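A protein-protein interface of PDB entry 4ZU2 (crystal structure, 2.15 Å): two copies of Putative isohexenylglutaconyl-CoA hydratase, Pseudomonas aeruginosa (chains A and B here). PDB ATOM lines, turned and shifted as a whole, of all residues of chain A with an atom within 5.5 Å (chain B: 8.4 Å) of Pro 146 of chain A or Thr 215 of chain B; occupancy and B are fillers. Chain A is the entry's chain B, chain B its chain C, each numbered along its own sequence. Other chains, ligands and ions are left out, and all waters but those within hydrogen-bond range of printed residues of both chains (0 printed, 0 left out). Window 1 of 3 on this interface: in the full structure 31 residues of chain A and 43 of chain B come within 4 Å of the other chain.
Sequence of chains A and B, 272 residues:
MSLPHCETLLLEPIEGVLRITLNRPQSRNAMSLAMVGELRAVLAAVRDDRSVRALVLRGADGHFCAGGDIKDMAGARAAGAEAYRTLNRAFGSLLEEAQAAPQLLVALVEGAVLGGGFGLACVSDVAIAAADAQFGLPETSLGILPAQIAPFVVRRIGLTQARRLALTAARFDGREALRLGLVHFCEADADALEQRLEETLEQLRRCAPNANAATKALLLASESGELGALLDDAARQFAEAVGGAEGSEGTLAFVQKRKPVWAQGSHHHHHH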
ATOM      1  N   LEU A 137     -27.194  15.572  -7.712  1.00  0.00           N
ATOM      2  CA  LEU A 137     -26.311  14.459  -7.423  1.00  0.00           C
ATOM      3  C   LEU A 137     -25.910  13.735  -8.720  1.00  0.00           C
ATOM      4  O   LEU A 137     -26.429  12.674  -9.036  1.00  0.00           O
ATOM      5  CB  LEU A 137     -27.006  13.488  -6.460  1.00  0.00           C
ATOM      6  CG  LEU A 137     -27.205  13.962  -5.016  1.00  0.00           C
ATOM      7  CD1 LEU A 137     -27.768  12.834  -4.152  1.00  0.00           C
ATOM      8  CD2 LEU A 137     -25.901  14.481  -4.424  1.00  0.00           C
ATOM      9  N   GLU A 139     -23.451  12.001  -9.564  1.00  0.00           N
ATOM     10  CA  GLU A 139     -22.538  10.893  -9.421  1.00  0.00           C
ATOM     11  C   GLU A 139     -22.760   9.669 -10.343  1.00  0.00           C
ATOM     12  O   GLU A 139     -21.809   9.117 -10.892  1.00  0.00           O
ATOM     13  CB  GLU A 139     -22.505  10.456  -7.948  1.00  0.00           C
ATOM     14  CG  GLU A 139     -21.555  11.294  -7.071  1.00  0.00           C
ATOM     15  CD  GLU A 139     -22.214  12.512  -6.419  1.00  0.00           C
ATOM     16  OE1 GLU A 139     -23.361  12.892  -6.788  1.00  0.00           O
ATOM     17  OE2 GLU A 139     -21.560  13.090  -5.502  1.00  0.00           O
ATOM     18  N   THR A 140     -23.997   9.231 -10.481  1.00  0.00           N
ATOM     19  CA  THR A 140     -24.273   8.006 -11.195  1.00  0.00           C
ATOM     20  C   THR A 140     -24.295   8.167 -12.740  1.00  0.00           C
ATOM     21  O   THR A 140     -24.059   7.202 -13.486  1.00  0.00           O
ATOM     22  CB  THR A 140     -25.564   7.415 -10.699  1.00  0.00           C
ATOM     23  OG1 THR A 140     -26.592   8.397 -10.756  1.00  0.00           O
ATOM     24  CG2 THR A 140     -25.405   6.948  -9.282  1.00  0.00           C
ATOM     25  N   ILE A 144     -20.410   6.784 -11.031  1.00  0.00           N
ATOM     26  CA  ILE A 144     -19.911   6.645  -9.656  1.00  0.00           C
ATOM     27  C   ILE A 144     -21.017   6.805  -8.582  1.00  0.00           C
ATOM     28  O   ILE A 144     -22.203   6.857  -8.908  1.00  0.00           O
ATOM     29  CB  ILE A 144     -18.740   7.621  -9.426  1.00  0.00           C
ATOM     30  CG1 ILE A 144     -19.211   9.083  -9.542  1.00  0.00           C
ATOM     31  CG2 ILE A 144     -17.647   7.349 -10.454  1.00  0.00           C
ATOM     32  CD1 ILE A 144     -18.118  10.146  -9.271  1.00  0.00           C
ATOM     33  N   LEU A 145     -20.623   6.885  -7.310  1.00  0.00           N
ATOM     34  CA  LEU A 145     -21.576   6.776  -6.191  1.00  0.00           C
ATOM     35  C   LEU A 145     -21.610   8.007  -5.296  1.00  0.00           C
ATOM     36  O   LEU A 145     -20.552   8.495  -4.876  1.00  0.00           O
ATOM     37  CB  LEU A 145     -21.196   5.583  -5.295  1.00  0.00           C
ATOM     38  CG  LEU A 145     -21.026   4.203  -5.925  1.00  0.00           C
ATOM     39  CD1 LEU A 145     -20.935   3.164  -4.828  1.00  0.00           C
ATOM     40  CD2 LEU A 145     -22.180   3.859  -6.848  1.00  0.00           C
ATOM     41  N   PRO A 146     -22.815   8.481  -4.940  1.00  0.00           N
ATOM     42  CA  PRO A 146     -22.935   9.503  -3.889  1.00  0.00           C
ATOM     43  C   PRO A 146     -22.815   8.759  -2.546  1.00  0.00           C
ATOM     44  O   PRO A 146     -23.758   8.575  -1.794  1.00  0.00           O
ATOM     45  CB  PRO A 146     -24.335  10.052  -4.123  1.00  0.00           C
ATOM     46  CG  PRO A 146     -25.073   8.859  -4.614  1.00  0.00           C
ATOM     47  CD  PRO A 146     -24.131   8.065  -5.433  1.00  0.00           C
ATOM     48  N   ALA A 147     -21.617   8.268  -2.296  1.00  0.00           N
ATOM     49  CA  ALA A 147     -21.441   7.146  -1.384  1.00  0.00           C
ATOM     50  C   ALA A 147     -21.502   7.617   0.054  1.00  0.00           C
ATOM     51  O   ALA A 147     -22.201   7.030   0.886  1.00  0.00           O
ATOM     52  CB  ALA A 147     -20.091   6.418  -1.685  1.00  0.00           C
ATOM     53  N   GLN A 148     -20.797   8.702   0.339  1.00  0.00           N
ATOM     54  CA  GLN A 148     -20.790   9.256   1.709  1.00  0.00           C
ATOM     55  C   GLN A 148     -22.026  10.107   1.953  1.00  0.00           C
ATOM     56  O   GLN A 148     -22.535  10.159   3.071  1.00  0.00           O
ATOM     57  CB  GLN A 148     -19.521  10.088   1.989  1.00  0.00           C
ATOM     58  CG  GLN A 148     -18.200   9.350   1.844  1.00  0.00           C
ATOM     59  CD  GLN A 148     -18.093   8.108   2.740  1.00  0.00           C
ATOM     60  OE1 GLN A 148     -17.761   8.184   3.940  1.00  0.00           O
ATOM     61  NE2 GLN A 148     -18.356   6.960   2.148  1.00  0.00           N
ATOM     62  N   ILE A 149     -22.507  10.755   0.896  1.00  0.00           N
ATOM     63  CA  ILE A 149     -23.695  11.574   0.999  1.00  0.00           C
ATOM     64  C   ILE A 149     -24.889  10.739   1.334  1.00  0.00           C
ATOM     65  O   ILE A 149     -25.740  11.186   2.078  1.00  0.00           O
ATOM     66  CB  ILE A 149     -23.995  12.328  -0.293  1.00  0.00           C
ATOM     67  CG1 ILE A 149     -22.860  13.302  -0.584  1.00  0.00           C
ATOM     68  CG2 ILE A 149     -25.328  13.069  -0.180  1.00  0.00           C
ATOM     69  CD1 ILE A 149     -22.989  14.079  -1.877  1.00  0.00           C
ATOM     70  N   ALA A 150     -24.961   9.541   0.750  1.00  0.00           N
ATOM     71  CA  ALA A 150     -26.163   8.689   0.842  1.00  0.00           C
ATOM     72  C   ALA A 150     -26.920   8.754   2.210  1.00  0.00           C
ATOM     73  O   ALA A 150     -28.058   9.168   2.272  1.00  0.00           O
ATOM     74  CB  ALA A 150     -25.826   7.222   0.451  1.00  0.00           C
ATOM     75  N   ALA A 166     -31.149  10.482  -6.535  1.00  0.00           N
ATOM     76  CA  ALA A 166     -29.890   9.754  -6.696  1.00  0.00           C
ATOM     77  C   ALA A 166     -29.879   8.837  -7.945  1.00  0.00           C
ATOM     78  O   ALA A 166     -28.850   8.653  -8.609  1.00  0.00           O
ATOM     79  CB  ALA A 166     -29.611   8.913  -5.436  1.00  0.00           C
ATOM     80  N   LEU A 167     -31.005   8.218  -8.236  1.00  0.00           N
ATOM     81  CA  LEU A 167     -31.033   7.232  -9.312  1.00  0.00           C
ATOM     82  C   LEU A 167     -31.400   7.830 -10.686  1.00  0.00           C
ATOM     83  O   LEU A 167     -31.223   7.170 -11.709  1.00  0.00           O
ATOM     84  CB  LEU A 167     -31.959   6.093  -8.937  1.00  0.00           C
ATOM     85  CG  LEU A 167     -31.595   5.440  -7.594  1.00  0.00           C
ATOM     86  CD1 LEU A 167     -32.506   4.250  -7.397  1.00  0.00           C
ATOM     87  CD2 LEU A 167     -30.095   5.057  -7.414  1.00  0.00           C
ATOM     88  N   PRO B 102     -32.920  -3.982  -7.721  1.00  0.00           N
ATOM     89  CA  PRO B 102     -31.788  -3.150  -8.156  1.00  0.00           C
ATOM     90  C   PRO B 102     -32.142  -2.238  -9.347  1.00  0.00           C
ATOM     91  O   PRO B 102     -31.340  -1.392  -9.737  1.00  0.00           O
ATOM     92  CB  PRO B 102     -30.728  -4.174  -8.568  1.00  0.00           C
ATOM     93  CG  PRO B 102     -31.156  -5.468  -7.885  1.00  0.00           C
ATOM     94  CD  PRO B 102     -32.641  -5.425  -7.824  1.00  0.00           C
ATOM     95  N   ALA B 208     -25.742   5.123 -14.994  1.00  0.00           N
ATOM     96  CA  ALA B 208     -25.236   3.767 -15.262  1.00  0.00           C
ATOM     97  C   ALA B 208     -25.770   2.749 -14.268  1.00  0.00           C
ATOM     98  O   ALA B 208     -25.852   3.015 -13.073  1.00  0.00           O
ATOM     99  CB  ALA B 208     -23.719   3.736 -15.247  1.00  0.00           C
ATOM    100  N   PRO B 209     -26.111   1.561 -14.765  1.00  0.00           N
ATOM    101  CA  PRO B 209     -26.952   0.637 -14.005  1.00  0.00           C
ATOM    102  C   PRO B 209     -26.302  -0.023 -12.794  1.00  0.00           C
ATOM    103  O   PRO B 209     -27.039  -0.372 -11.871  1.00  0.00           O
ATOM    104  CB  PRO B 209     -27.305  -0.425 -15.041  1.00  0.00           C
ATOM    105  CG  PRO B 209     -26.207  -0.385 -15.989  1.00  0.00           C
ATOM    106  CD  PRO B 209     -25.839   1.046 -16.111  1.00  0.00           C
ATOM    107  N   ASN B 210     -24.988  -0.239 -12.821  1.00  0.00           N
ATOM    108  CA  ASN B 210     -24.319  -0.805 -11.660  1.00  0.00           C
ATOM    109  C   ASN B 210     -24.205   0.260 -10.562  1.00  0.00           C
ATOM    110  O   ASN B 210     -24.427  -0.032  -9.404  1.00  0.00           O
ATOM    111  CB  ASN B 210     -22.953  -1.411 -11.996  1.00  0.00           C
ATOM    112  CG  ASN B 210     -23.062  -2.780 -12.650  1.00  0.00           C
ATOM    113  OD1 ASN B 210     -23.466  -3.747 -12.022  1.00  0.00           O
ATOM    114  ND2 ASN B 210     -22.689  -2.864 -13.915  1.00  0.00           N
ATOM    115  N   ALA B 211     -23.877   1.488 -10.962  1.00  0.00           N
ATOM    116  CA  ALA B 211     -23.848   2.631 -10.055  1.00  0.00           C
ATOM    117  C   ALA B 211     -25.194   2.824  -9.377  1.00  0.00           C
ATOM    118  O   ALA B 211     -25.244   3.084  -8.181  1.00  0.00           O
ATOM    119  CB  ALA B 211     -23.454   3.912 -10.799  1.00  0.00           C
ATOM    120  N   ASN B 212     -26.282   2.675 -10.130  1.00  0.00           N
ATOM    121  CA  ASN B 212     -27.595   2.867  -9.552  1.00  0.00           C
ATOM    122  C   ASN B 212     -28.005   1.736  -8.590  1.00  0.00           C
ATOM    123  O   ASN B 212     -28.687   1.976  -7.585  1.00  0.00           O
ATOM    124  CB  ASN B 212     -28.633   3.078 -10.648  1.00  0.00           C
ATOM    125  CG  ASN B 212     -28.851   4.545 -10.966  1.00  0.00           C
ATOM    126  OD1 ASN B 212     -28.024   5.402 -10.636  1.00  0.00           O
ATOM    127  ND2 ASN B 212     -29.958   4.841 -11.614  1.00  0.00           N
ATOM    128  N   ALA B 213     -27.543   0.521  -8.860  1.00  0.00           N
ATOM    129  CA  ALA B 213     -27.858  -0.602  -7.991  1.00  0.00           C
ATOM    130  C   ALA B 213     -27.142  -0.460  -6.666  1.00  0.00           C
ATOM    131  O   ALA B 213     -27.724  -0.710  -5.618  1.00  0.00           O
ATOM    132  CB  ALA B 213     -27.480  -1.910  -8.643  1.00  0.00           C
ATOM    133  N   ALA B 214     -25.875  -0.063  -6.720  1.00  0.00           N
ATOM    134  CA  ALA B 214     -25.063   0.064  -5.519  1.00  0.00           C
ATOM    135  C   ALA B 214     -25.534   1.231  -4.643  1.00  0.00           C
ATOM    136  O   ALA B 214     -25.564   1.128  -3.410  1.00  0.00           O
ATOM    137  CB  ALA B 214     -23.625   0.250  -5.903  1.00  0.00           C
ATOM    138  N   THR B 215     -25.878   2.341  -5.294  1.00  0.00           N
ATOM    139  CA  THR B 215     -26.428   3.522  -4.624  1.00  0.00           C
ATOM    140  C   THR B 215     -27.749   3.198  -3.905  1.00  0.00           C
ATOM    141  O   THR B 215     -27.887   3.440  -2.720  1.00  0.00           O
ATOM    142  CB  THR B 215     -26.653   4.610  -5.646  1.00  0.00           C
ATOM    143  OG1 THR B 215     -25.386   5.001  -6.170  1.00  0.00           O
ATOM    144  CG2 THR B 215     -27.367   5.820  -5.045  1.00  0.00           C
ATOM    145  N   LYS B 216     -28.694   2.618  -4.635  1.00  0.00           N
ATOM    146  CA  LYS B 216     -29.951   2.202  -4.041  1.00  0.00           C
ATOM    147  C   LYS B 216     -29.768   1.318  -2.815  1.00  0.00           C
ATOM    148  O   LYS B 216     -30.466   1.500  -1.833  1.00  0.00           O
ATOM    149  CB  LYS B 216     -30.824   1.496  -5.068  1.00  0.00           C
ATOM    150  CG  LYS B 216     -32.096   0.939  -4.513  1.00  0.00           C
ATOM    151  CD  LYS B 216     -33.190   0.952  -5.571  1.00  0.00           C
ATOM    152  CE  LYS B 216     -34.396   0.125  -5.179  1.00  0.00           C
ATOM    153  NZ  LYS B 216     -35.447   0.133  -6.198  1.00  0.00           N
ATOM    154  N   ALA B 217     -28.831   0.379  -2.868  1.00  0.00           N
ATOM    155  CA  ALA B 217     -28.528  -0.466  -1.719  1.00  0.00           C
ATOM    156  C   ALA B 217     -28.047   0.352  -0.512  1.00  0.00           C
ATOM    157  O   ALA B 217     -28.483   0.122   0.600  1.00  0.00           O
ATOM    158  CB  ALA B 217     -27.473  -1.471  -2.102  1.00  0.00           C
ATOM    159  N   LEU B 218     -27.121   1.275  -0.747  1.00  0.00           N
ATOM    160  CA  LEU B 218     -26.615   2.186   0.287  1.00  0.00           C
ATOM    161  C   LEU B 218     -27.767   2.958   0.898  1.00  0.00           C
ATOM    162  O   LEU B 218     -27.982   2.908   2.083  1.00  0.00           O
ATOM    163  CB  LEU B 218     -25.630   3.195  -0.330  1.00  0.00           C
ATOM    164  CG  LEU B 218     -24.114   2.967  -0.231  1.00  0.00           C
ATOM    165  CD1 LEU B 218     -23.739   1.509  -0.192  1.00  0.00           C
ATOM    166  CD2 LEU B 218     -23.381   3.643  -1.397  1.00  0.00           C
ATOM    167  N   LEU B 219     -28.497   3.673   0.055  1.00  0.00           N
ATOM    168  CA  LEU B 219     -29.696   4.376   0.453  1.00  0.00           C
ATOM    169  C   LEU B 219     -30.585   3.533   1.348  1.00  0.00           C
ATOM    170  O   LEU B 219     -30.954   3.971   2.442  1.00  0.00           O
ATOM    171  CB  LEU B 219     -30.503   4.793  -0.784  1.00  0.00           C
ATOM    172  CG  LEU B 219     -29.966   5.903  -1.695  1.00  0.00           C
ATOM    173  CD1 LEU B 219     -31.045   6.280  -2.651  1.00  0.00           C
ATOM    174  CD2 LEU B 219     -29.481   7.170  -0.948  1.00  0.00           C
ATOM    175  N   LEU B 220     -30.937   2.332   0.892  1.00  0.00           N
ATOM    176  CA  LEU B 220     -31.851   1.478   1.669  1.00  0.00           C
ATOM    177  C   LEU B 220     -31.273   1.067   3.043  1.00  0.00           C
ATOM    178  O   LEU B 220     -32.022   0.885   3.997  1.00  0.00           O
ATOM    179  CB  LEU B 220     -32.307   0.263   0.863  1.00  0.00           C
ATOM    180  CG  LEU B 220     -33.324   0.536  -0.267  1.00  0.00           C
ATOM    181  CD1 LEU B 220     -33.560  -0.749  -1.058  1.00  0.00           C
ATOM    182  CD2 LEU B 220     -34.649   1.077   0.258  1.00  0.00           C
ATOM    183  N   ALA B 221     -29.951   0.995   3.141  1.00  0.00           N
ATOM    184  CA  ALA B 221     -29.278   0.524   4.341  1.00  0.00           C
ATOM    185  C   ALA B 221     -28.933   1.674   5.309  1.00  0.00           C
ATOM    186  O   ALA B 221     -28.391   1.429   6.381  1.00  0.00           O
ATOM    187  CB  ALA B 221     -27.993  -0.286   3.972  1.00  0.00           C
ATOM    188  N   SER B 222     -29.257   2.912   4.940  1.00  0.00           N
ATOM    189  CA  SER B 222     -28.939   4.076   5.777  1.00  0.00           C
ATOM    190  C   SER B 222     -29.918   4.231   6.932  1.00  0.00           C
ATOM    191  O   SER B 222     -29.564   4.486   8.094  1.00  0.00           O
ATOM    192  CB  SER B 222     -29.008   5.351   4.945  1.00  0.00           C
ATOM    193  OG  SER B 222     -28.696   5.101   3.603  1.00  0.00           O
ATOM    194  N   LEU B 231     -20.344   4.092   6.362  1.00  0.00           N
ATOM    195  CA  LEU B 231     -19.461   4.976   5.617  1.00  0.00           C
ATOM    196  C   LEU B 231     -18.176   4.253   5.241  1.00  0.00           C
ATOM    197  O   LEU B 231     -17.672   4.419   4.127  1.00  0.00           O
ATOM    198  CB  LEU B 231     -19.173   6.270   6.399  1.00  0.00           C
ATOM    199  CG  LEU B 231     -20.374   7.215   6.567  1.00  0.00           C
ATOM    200  CD1 LEU B 231     -20.006   8.344   7.455  1.00  0.00           C
ATOM    201  CD2 LEU B 231     -20.872   7.761   5.243  1.00  0.00           C
ATOM    202  N   ALA B 234     -19.276   1.975   2.255  1.00  0.00           N
ATOM    203  CA  ALA B 234     -19.564   2.846   1.113  1.00  0.00           C
ATOM    204  C   ALA B 234     -18.304   3.410   0.465  1.00  0.00           C
ATOM    205  O   ALA B 234     -18.263   3.669  -0.744  1.00  0.00           O
ATOM    206  CB  ALA B 234     -20.467   4.006   1.551  1.00  0.00           C
ATOM    207  N   GLN B 237     -16.778   0.730  -1.704  1.00  0.00           N
ATOM    208  CA  GLN B 237     -17.614   0.707  -2.892  1.00  0.00           C
ATOM    209  C   GLN B 237     -17.331   1.893  -3.812  1.00  0.00           C
ATOM    210  O   GLN B 237     -17.316   1.752  -5.032  1.00  0.00           O
ATOM    211  CB  GLN B 237     -19.094   0.681  -2.474  1.00  0.00           C
ATOM    212  CG  GLN B 237     -19.512  -0.656  -1.904  1.00  0.00           C
ATOM    213  CD  GLN B 237     -21.011  -0.759  -1.670  1.00  0.00           C
ATOM    214  OE1 GLN B 237     -21.806  -0.350  -2.508  1.00  0.00           O
ATOM    215  NE2 GLN B 237     -21.397  -1.308  -0.526  1.00  0.00           N
ATOM    216  N   PHE B 238     -17.123   3.067  -3.231  1.00  0.00           N
ATOM    217  CA  PHE B 238     -16.845   4.248  -4.028  1.00  0.00           C
ATOM    218  C   PHE B 238     -15.567   4.054  -4.860  1.00  0.00           C
ATOM    219  O   PHE B 238     -15.509   4.441  -6.017  1.00  0.00           O
ATOM    220  CB  PHE B 238     -16.714   5.484  -3.141  1.00  0.00           C
ATOM    221  CG  PHE B 238     -16.357   6.717  -3.898  1.00  0.00           C
ATOM    222  CD1 PHE B 238     -17.324   7.432  -4.577  1.00  0.00           C
ATOM    223  CD2 PHE B 238     -15.056   7.148  -3.959  1.00  0.00           C
ATOM    224  CE1 PHE B 238     -16.990   8.569  -5.298  1.00  0.00           C
ATOM    225  CE2 PHE B 238     -14.717   8.280  -4.673  1.00  0.00           C
ATOM    226  CZ  PHE B 238     -15.687   8.996  -5.340  1.00  0.00           C
ATOM    227  N   ALA B 241     -16.313   1.672  -7.866  1.00  0.00           N
ATOM    228  CA  ALA B 241     -17.048   2.315  -8.939  1.00  0.00           C
ATOM    229  C   ALA B 241     -16.109   3.220  -9.739  1.00  0.00           C
ATOM    230  O   ALA B 241     -16.146   3.220 -10.968  1.00  0.00           O
ATOM    231  CB  ALA B 241     -18.191   3.096  -8.391  1.00  0.00           C
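Among the printed residues, no Asp or Glu carboxylate lies within 4 Å of a Lys or Arg side-chain nitrogen of the other chain.
Pro 146 of chain A touches just one residue of chain B: Thr 215. Pro 209 of chain B touches none of the printed residues of chain A. Asn 210 of chain B touches none of the printed residues of chain A. Of the printed residues of chain A, Ala 211 of chain B touches Thr 140 (3.9 Å), Ile 144 (3.7 Å) and Leu 145 (3.4 Å). Of the printed residues of chain A, Asn 212 of chain B touches Thr 140, Ala 166 and Leu 167. The nearest printed residue of chain A that does not touch Ala 234 of chain B is Leu 145 of chain A (4.9 Å).
CG2 of Thr 140 of chain A touches CB of Ala 211 of chain B, at 3.9 Å. Thr 140 of chain A touches Thr 215 of chain B. Ala 211 of chain B touches Ile 144 of chain A (CB to O, 3.7 Å). CD1 of Leu 145 of chain A touches CB of Gln 237 of chain B, at 3.9 Å. Leu 145 of chain A touches Phe 238 of chain B. Pro 146 of chain A touches Thr 215 of chain B. Phe 238 of chain B touches Ala 147 of chain A (CB to CB, 3.8 Å). NE2 of Gln 148 of chain A touches CB of Ala 234 of chain B, at 3.7 Å. CG2 of Thr 215 of chain B touches CB of Ala 166 of chain A (3.8 Å). Leu 167 of chain A touches Lys 216 of chain B (CD1 to CD, 3.8 Å).
No position is printed for both chains.
O of Ala 166 of chain A is in hydrogen-bond range of OG1 of Thr 140 of chain A (3.1 Å). The backbone NH (N) of Ile 144 of chain A lies within hydrogen-bond range of the backbone carbonyl oxygen (O) of Glu 139 of chain A (2.7 Å). The backbone carbonyl oxygen (O) of Ala 211 of chain B is in hydrogen-bond range of the side-chain hydroxyl (OG1) of Thr 215 of chain B, at 2.8 Å. The backbone carbonyl oxygen (O) of Leu 219 of chain B is in hydrogen-bond range of the side-chain hydroxyl (OG) of Ser 222 of chain B, 2.8 Å away.
The backbone carbonyl oxygen of Leu 231 of chain B sits at hydrogen-bond distance from the side-chain amide nitrogen of Gln 148 of chain A (3.3 Å). O of Thr 140 of chain A sits at hydrogen-bond distance from N of Ala 208 of chain B (3.1 Å). O of Leu 167 of chain A is in hydrogen-bond range of ND2 of Asn 212 of chain B (2.7 Å). The side-chain hydroxyl (OG1) of Thr 140 of chain A lies close to the side-chain amide oxygen (OD1) of Asn 212 of chain B, 3.3 Å away.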
